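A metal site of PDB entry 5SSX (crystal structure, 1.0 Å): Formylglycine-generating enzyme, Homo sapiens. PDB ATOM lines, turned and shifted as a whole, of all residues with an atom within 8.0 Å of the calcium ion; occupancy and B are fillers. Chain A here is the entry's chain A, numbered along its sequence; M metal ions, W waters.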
ATOM      1  N   HIS A 193       1.415   2.097  -8.688  1.00  0.00           N
ATOM      2  CA  HIS A 193       0.124   1.576  -8.257  1.00  0.00           C
ATOM      3  C   HIS A 193       0.021   0.111  -8.630  1.00  0.00           C
ATOM      4  O   HIS A 193       0.309  -0.280  -9.748  1.00  0.00           O
ATOM      5  CB  HIS A 193      -1.019   2.385  -8.847  1.00  0.00           C
ATOM      6  CG  HIS A 193      -1.185   3.714  -8.185  1.00  0.00           C
ATOM      7  ND1 HIS A 193      -1.794   3.837  -6.961  1.00  0.00           N
ATOM      8  CD2 HIS A 193      -0.744   4.954  -8.521  1.00  0.00           C
ATOM      9  CE1 HIS A 193      -1.723   5.100  -6.581  1.00  0.00           C
ATOM     10  NE2 HIS A 193      -1.091   5.793  -7.507  1.00  0.00           N
ATOM     11  N   ALA A 195      -2.949  -1.724  -7.535  1.00  0.00           N
ATOM     12  CA  ALA A 195      -4.363  -2.079  -7.465  1.00  0.00           C
ATOM     13  C   ALA A 195      -5.184  -0.826  -7.684  1.00  0.00           C
ATOM     14  O   ALA A 195      -4.718   0.315  -7.442  1.00  0.00           O
ATOM     15  CB  ALA A 195      -4.723  -2.691  -6.122  1.00  0.00           C
ATOM     16  N   ASN A 196      -6.423  -1.018  -8.119  1.00  0.00           N
ATOM     17  CA  ASN A 196      -7.371   0.043  -8.381  1.00  0.00           C
ATOM     18  C   ASN A 196      -8.229   0.286  -7.155  1.00  0.00           C
ATOM     19  O   ASN A 196      -9.187  -0.454  -6.892  1.00  0.00           O
ATOM     20  CB  ASN A 196      -8.232  -0.347  -9.569  1.00  0.00           C
ATOM     21  CG  ASN A 196      -9.266   0.714  -9.897  1.00  0.00           C
ATOM     22  OD1 ASN A 196      -9.113   1.882  -9.517  1.00  0.00           O
ATOM     23  ND2 ASN A 196     -10.285   0.329 -10.629  1.00  0.00           N
ATOM     24  N   ILE A 197      -7.888   1.311  -6.396  1.00  0.00           N
ATOM     25  CA  ILE A 197      -8.668   1.775  -5.269  1.00  0.00           C
ATOM     26  C   ILE A 197      -8.923   3.274  -5.450  1.00  0.00           C
ATOM     27  O   ILE A 197      -8.782   3.797  -6.546  1.00  0.00           O
ATOM     28  CB  ILE A 197      -8.024   1.382  -3.916  1.00  0.00           C
ATOM     29  CG1 ILE A 197      -6.650   2.003  -3.716  1.00  0.00           C
ATOM     30  CG2 ILE A 197      -7.992  -0.148  -3.808  1.00  0.00           C
ATOM     31  CD1 ILE A 197      -6.122   1.770  -2.304  1.00  0.00           C
ATOM     32  N   TRP A 198      -9.332   3.960  -4.400  1.00  0.00           N
ATOM     33  CA  TRP A 198      -9.628   5.390  -4.462  1.00  0.00           C
ATOM     34  C   TRP A 198      -8.379   6.190  -4.114  1.00  0.00           C
ATOM     35  O   TRP A 198      -7.646   5.819  -3.216  1.00  0.00           O
ATOM     36  CB  TRP A 198     -10.693   5.704  -3.426  1.00  0.00           C
ATOM     37  CG  TRP A 198     -11.305   7.058  -3.458  1.00  0.00           C
ATOM     38  CD1 TRP A 198     -10.823   8.203  -2.918  1.00  0.00           C
ATOM     39  CD2 TRP A 198     -12.589   7.384  -3.998  1.00  0.00           C
ATOM     40  NE1 TRP A 198     -11.724   9.221  -3.090  1.00  0.00           N
ATOM     41  CE2 TRP A 198     -12.805   8.748  -3.771  1.00  0.00           C
ATOM     42  CE3 TRP A 198     -13.560   6.653  -4.679  1.00  0.00           C
ATOM     43  CZ2 TRP A 198     -13.982   9.396  -4.150  1.00  0.00           C
ATOM     44  CZ3 TRP A 198     -14.726   7.291  -5.075  1.00  0.00           C
ATOM     45  CH2 TRP A 198     -14.937   8.648  -4.793  1.00  0.00           C
ATOM     46  N   GLN A 199      -8.173   7.308  -4.789  1.00  0.00           N
ATOM     47  CA  GLN A 199      -7.235   8.329  -4.318  1.00  0.00           C
ATOM     48  C   GLN A 199      -7.995   9.642  -4.232  1.00  0.00           C
ATOM     49  O   GLN A 199      -8.846   9.929  -5.063  1.00  0.00           O
ATOM     50  CB  GLN A 199      -6.001   8.519  -5.209  1.00  0.00           C
ATOM     51  CG  GLN A 199      -5.132   7.299  -5.302  1.00  0.00           C
ATOM     52  CD  GLN A 199      -5.624   6.317  -6.357  1.00  0.00           C
ATOM     53  OE1 GLN A 199      -6.054   6.711  -7.451  1.00  0.00           O
ATOM     54  NE2 GLN A 199      -5.538   5.033  -6.055  1.00  0.00           N
ATOM     55  N   ASN A 206     -12.455  11.602  -6.326  1.00  0.00           N
ATOM     56  CA  ASN A 206     -11.562  10.515  -6.714  1.00  0.00           C
ATOM     57  C   ASN A 206     -10.664  11.096  -7.796  1.00  0.00           C
ATOM     58  O   ASN A 206     -11.140  11.463  -8.879  1.00  0.00           O
ATOM     59  CB  ASN A 206     -12.360   9.337  -7.247  1.00  0.00           C
ATOM     60  CG  ASN A 206     -11.492   8.115  -7.486  1.00  0.00           C
ATOM     61  OD1 ASN A 206     -10.255   8.190  -7.439  1.00  0.00           O
ATOM     62  ND2 ASN A 206     -12.127   6.991  -7.758  1.00  0.00           N
ATOM     63  N   THR A 207      -9.376  11.196  -7.506  1.00  0.00           N
ATOM     64  CA  THR A 207      -8.471  11.829  -8.454  1.00  0.00           C
ATOM     65  C   THR A 207      -8.174  10.944  -9.655  1.00  0.00           C
ATOM     66  O   THR A 207      -7.664  11.443 -10.644  1.00  0.00           O
ATOM     67  CB  THR A 207      -7.144  12.211  -7.800  1.00  0.00           C
ATOM     68  OG1 THR A 207      -6.492  10.993  -7.444  1.00  0.00           O
ATOM     69  CG2 THR A 207      -7.373  13.097  -6.578  1.00  0.00           C
ATOM     70  N   GLY A 208      -8.399   9.621  -9.564  1.00  0.00           N
ATOM     71  CA  GLY A 208      -8.027   8.776 -10.664  1.00  0.00           C
ATOM     72  C   GLY A 208      -6.534   8.666 -10.883  1.00  0.00           C
ATOM     73  O   GLY A 208      -6.091   8.311 -11.970  1.00  0.00           O
ATOM     74  N   GLU A 209      -5.755   8.916  -9.834  1.00  0.00           N
ATOM     75  CA  GLU A 209      -4.308   8.847  -9.924  1.00  0.00           C
ATOM     76  C   GLU A 209      -3.830   7.485 -10.420  1.00  0.00           C
ATOM     77  O   GLU A 209      -2.878   7.414 -11.185  1.00  0.00           O
ATOM     78  CB  GLU A 209      -3.719   9.135  -8.546  1.00  0.00           C
ATOM     79  CG  GLU A 209      -2.230   9.026  -8.475  1.00  0.00           C
ATOM     80  CD  GLU A 209      -1.719   9.091  -7.049  1.00  0.00           C
ATOM     81  OE1 GLU A 209      -2.398   9.667  -6.163  1.00  0.00           O
ATOM     82  OE2 GLU A 209      -0.624   8.514  -6.804  1.00  0.00           O
ATOM     83  N   ASP A 210      -4.479   6.401 -10.000  1.00  0.00           N
ATOM     84  CA  ASP A 210      -4.061   5.059 -10.411  1.00  0.00           C
ATOM     85  C   ASP A 210      -4.524   4.689 -11.809  1.00  0.00           C
ATOM     86  O   ASP A 210      -4.256   3.562 -12.239  1.00  0.00           O
ATOM     87  CB  ASP A 210      -4.540   4.001  -9.391  1.00  0.00           C
ATOM     88  CG  ASP A 210      -6.049   3.902  -9.274  1.00  0.00           C
ATOM     89  OD1 ASP A 210      -6.771   4.321 -10.204  1.00  0.00           O
ATOM     90  OD2 ASP A 210      -6.521   3.384  -8.222  1.00  0.00           O
ATOM     91  N   GLY A 211      -5.161   5.600 -12.523  1.00  0.00           N
ATOM     92  CA  GLY A 211      -5.572   5.373 -13.886  1.00  0.00           C
ATOM     93  C   GLY A 211      -7.021   5.017 -14.097  1.00  0.00           C
ATOM     94  O   GLY A 211      -7.446   4.935 -15.246  1.00  0.00           O
ATOM     95  N   PHE A 212      -7.804   4.839 -13.025  1.00  0.00           N
ATOM     96  CA  PHE A 212      -9.184   4.373 -13.134  1.00  0.00           C
ATOM     97  C   PHE A 212     -10.026   4.984 -12.036  1.00  0.00           C
ATOM     98  O   PHE A 212      -9.712   4.830 -10.859  1.00  0.00           O
ATOM     99  CB  PHE A 212      -9.267   2.842 -13.069  1.00  0.00           C
ATOM    100  CG  PHE A 212      -8.431   2.204 -14.115  1.00  0.00           C
ATOM    101  CD1 PHE A 212      -8.920   2.008 -15.398  1.00  0.00           C
ATOM    102  CD2 PHE A 212      -7.118   1.874 -13.847  1.00  0.00           C
ATOM    103  CE1 PHE A 212      -8.079   1.486 -16.388  1.00  0.00           C
ATOM    104  CE2 PHE A 212      -6.304   1.343 -14.803  1.00  0.00           C
ATOM    105  CZ  PHE A 212      -6.764   1.170 -16.069  1.00  0.00           C
ATOM    106  N   GLN A 213     -11.114   5.636 -12.432  1.00  0.00           N
ATOM    107  CA  GLN A 213     -12.059   6.092 -11.435  1.00  0.00           C
ATOM    108  C   GLN A 213     -13.054   5.016 -11.052  1.00  0.00           C
ATOM    109  O   GLN A 213     -13.184   4.759  -9.859  1.00  0.00           O
ATOM    110  CB  GLN A 213     -12.721   7.389 -11.831  1.00  0.00           C
ATOM    111  CG  GLN A 213     -11.705   8.521 -11.826  1.00  0.00           C
ATOM    112  CD  GLN A 213     -12.215   9.755 -12.466  1.00  0.00           C
ATOM    113  OE1 GLN A 213     -12.786   9.694 -13.544  1.00  0.00           O
ATOM    114  NE2 GLN A 213     -12.015  10.906 -11.810  1.00  0.00           N
ATOM    115  N   GLY A 214     -13.713   4.385 -11.985  1.00  0.00           N
ATOM    116  CA  GLY A 214     -14.504   3.195 -11.754  1.00  0.00           C
ATOM    117  C   GLY A 214     -13.627   1.980 -11.897  1.00  0.00           C
ATOM    118  O   GLY A 214     -12.435   2.006 -11.556  1.00  0.00           O
ATOM    119  N   THR A 215     -14.184   0.900 -12.421  1.00  0.00           N
ATOM    120  CA  THR A 215     -13.402  -0.305 -12.613  1.00  0.00           C
ATOM    121  C   THR A 215     -12.333  -0.109 -13.677  1.00  0.00           C
ATOM    122  O   THR A 215     -12.413   0.771 -14.541  1.00  0.00           O
ATOM    123  CB  THR A 215     -14.308  -1.481 -13.010  1.00  0.00           C
ATOM    124  OG1 THR A 215     -15.042  -1.138 -14.198  1.00  0.00           O
ATOM    125  CG2 THR A 215     -15.276  -1.874 -11.880  1.00  0.00           C
ATOM    126  N   ALA A 216     -11.372  -0.997 -13.623  1.00  0.00           N
ATOM    127  CA  ALA A 216     -10.345  -1.216 -14.626  1.00  0.00           C
ATOM    128  C   ALA A 216     -10.633  -2.539 -15.346  1.00  0.00           C
ATOM    129  O   ALA A 216     -11.306  -3.420 -14.792  1.00  0.00           O
ATOM    130  CB  ALA A 216      -8.976  -1.317 -13.953  1.00  0.00           C
ATOM    131  N   PHE A 221      -3.136  -3.959 -14.039  1.00  0.00           N
ATOM    132  CA  PHE A 221      -2.229  -3.954 -12.892  1.00  0.00           C
ATOM    133  C   PHE A 221      -1.374  -5.210 -12.860  1.00  0.00           C
ATOM    134  O   PHE A 221      -1.657  -6.174 -13.576  1.00  0.00           O
ATOM    135  CB  PHE A 221      -2.967  -3.681 -11.571  1.00  0.00           C
ATOM    136  CG  PHE A 221      -3.535  -2.297 -11.509  1.00  0.00           C
ATOM    137  CD1 PHE A 221      -2.721  -1.214 -11.235  1.00  0.00           C
ATOM    138  CD2 PHE A 221      -4.855  -2.045 -11.825  1.00  0.00           C
ATOM    139  CE1 PHE A 221      -3.224   0.063 -11.229  1.00  0.00           C
ATOM    140  CE2 PHE A 221      -5.333  -0.774 -11.853  1.00  0.00           C
ATOM    141  CZ  PHE A 221      -4.534   0.283 -11.550  1.00  0.00           C
ATOM    142  N   ASN A 234     -10.480  -2.976  -7.347  1.00  0.00           N
ATOM    143  CA  ASN A 234     -11.268  -3.122  -8.575  1.00  0.00           C
ATOM    144  C   ASN A 234     -12.711  -3.436  -8.235  1.00  0.00           C
ATOM    145  O   ASN A 234     -13.544  -2.521  -8.222  1.00  0.00           O
ATOM    146  CB  ASN A 234     -10.627  -4.046  -9.622  1.00  0.00           C
ATOM    147  CG  ASN A 234     -10.905  -3.588 -11.032  1.00  0.00           C
ATOM    148  OD1 ASN A 234     -11.084  -2.392 -11.250  1.00  0.00           O
ATOM    149  ND2 ASN A 234     -10.927  -4.506 -11.989  1.00  0.00           N
ATOM    150  N   SER A 270     -12.573  -2.809  -3.465  1.00  0.00           N
ATOM    151  CA  SER A 270     -13.007  -2.340  -4.774  1.00  0.00           C
ATOM    152  C   SER A 270     -12.328  -1.016  -5.101  1.00  0.00           C
ATOM    153  O   SER A 270     -11.572  -0.442  -4.302  1.00  0.00           O
ATOM    154  CB  SER A 270     -14.519  -2.140  -4.860  1.00  0.00           C
ATOM    155  OG  SER A 270     -14.925  -0.939  -4.225  1.00  0.00           O
ATOM    156  N   TYR A 271     -12.672  -0.474  -6.265  1.00  0.00           N
ATOM    157  CA  TYR A 271     -12.214   0.833  -6.715  1.00  0.00           C
ATOM    158  C   TYR A 271     -12.625   1.963  -5.785  1.00  0.00           C
ATOM    159  O   TYR A 271     -12.068   3.056  -5.898  1.00  0.00           O
ATOM    160  CB  TYR A 271     -12.718   1.083  -8.122  1.00  0.00           C
ATOM    161  CG  TYR A 271     -14.193   1.360  -8.286  1.00  0.00           C
ATOM    162  CD1 TYR A 271     -14.708   2.602  -8.010  1.00  0.00           C
ATOM    163  CD2 TYR A 271     -15.042   0.380  -8.776  1.00  0.00           C
ATOM    164  CE1 TYR A 271     -16.043   2.909  -8.219  1.00  0.00           C
ATOM    165  CE2 TYR A 271     -16.393   0.675  -8.990  1.00  0.00           C
ATOM    166  CZ  TYR A 271     -16.863   1.945  -8.723  1.00  0.00           C
ATOM    167  OH  TYR A 271     -18.182   2.256  -8.960  1.00  0.00           O
ATOM    168  N   MET A 272     -13.562   1.717  -4.866  1.00  0.00           N
ATOM    169  CA  MET A 272     -13.981   2.705  -3.896  1.00  0.00           C
ATOM    170  C   MET A 272     -13.153   2.728  -2.626  1.00  0.00           C
ATOM    171  O   MET A 272     -13.292   3.688  -1.855  1.00  0.00           O
ATOM    172  CB  MET A 272     -15.436   2.452  -3.480  1.00  0.00           C
ATOM    173  CG  MET A 272     -16.415   2.612  -4.609  1.00  0.00           C
ATOM    174  SD  MET A 272     -18.072   2.075  -4.167  1.00  0.00           S
ATOM    175  CE  MET A 272     -18.479   3.206  -2.828  1.00  0.00           C
ATOM    176  N   CYS A 273     -12.338   1.730  -2.356  1.00  0.00           N
ATOM    177  CA  CYS A 273     -11.707   1.648  -1.041  1.00  0.00           C
ATOM    178  C   CYS A 273     -10.720   2.783  -0.815  1.00  0.00           C
ATOM    179  O   CYS A 273      -9.997   3.178  -1.702  1.00  0.00           O
ATOM    180  CB  CYS A 273     -10.944   0.354  -0.877  1.00  0.00           C
ATOM    181  SG  CYS A 273     -11.871  -1.170  -0.648  1.00  0.00           S
HETATM  182 CA    CA M   1      -8.792   4.053  -8.864  1.00  0.00          CA
HETATM  183  O   HOH W   1     -11.072   4.259  -8.190  1.00  0.00           O
HETATM  184  O   HOH W   2      -8.533   6.341  -8.406  1.00  0.00           O
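The side-chain amide nitrogen (ND2) of Asn 196 sits close to the backbone NH (N) of Ala 216, 3.5 Å away. The backbone NH (N) of Asn 234 is in hydrogen-bond range of the backbone carbonyl oxygen (O) of Asn 196 (2.9 Å). The backbone NH (N) of Asp 210 is in hydrogen-bond range of the side-chain amide oxygen (OE1) of Gln 199 (3.0 Å). O of Gly 214 is in hydrogen-bond range of ND2 of Asn 196 (2.9 Å).
Of the 23 residues printed, 4 come within 4 Å of the calcium ion. The nearest printed residue that does not touch the calcium ion is Gln 199 (4.1 Å).
The calcium ion is bound by the side-chain amide oxygen (OD1) of Asn 196 (2.3 Å), the backbone carbonyl oxygen (O) of Phe 212 (2.3 Å), the backbone carbonyl oxygen (O) of Ile 197 (2.3 Å), water W2 (2.3 Å), water W1 (2.4 Å), the side-chain carboxylate (OD1) of Asp 210 (2.4 Å) and the side-chain carboxylate (OD2) of Asp 210 (2.5 Å).
Water W1 lies within hydrogen-bond range of the backbone carbonyl oxygen of Gln 213 (2.7 Å), the backbone carbonyl oxygen of Tyr 271 (2.8 Å) and the side-chain amide nitrogen of Asn 206 (3.0 Å). Water W2 lies within hydrogen-bond range of OE1 of Gln 199 (2.7 Å), OD1 of Asn 206 (2.7 Å) and N of Gly 208 (3.5 Å).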
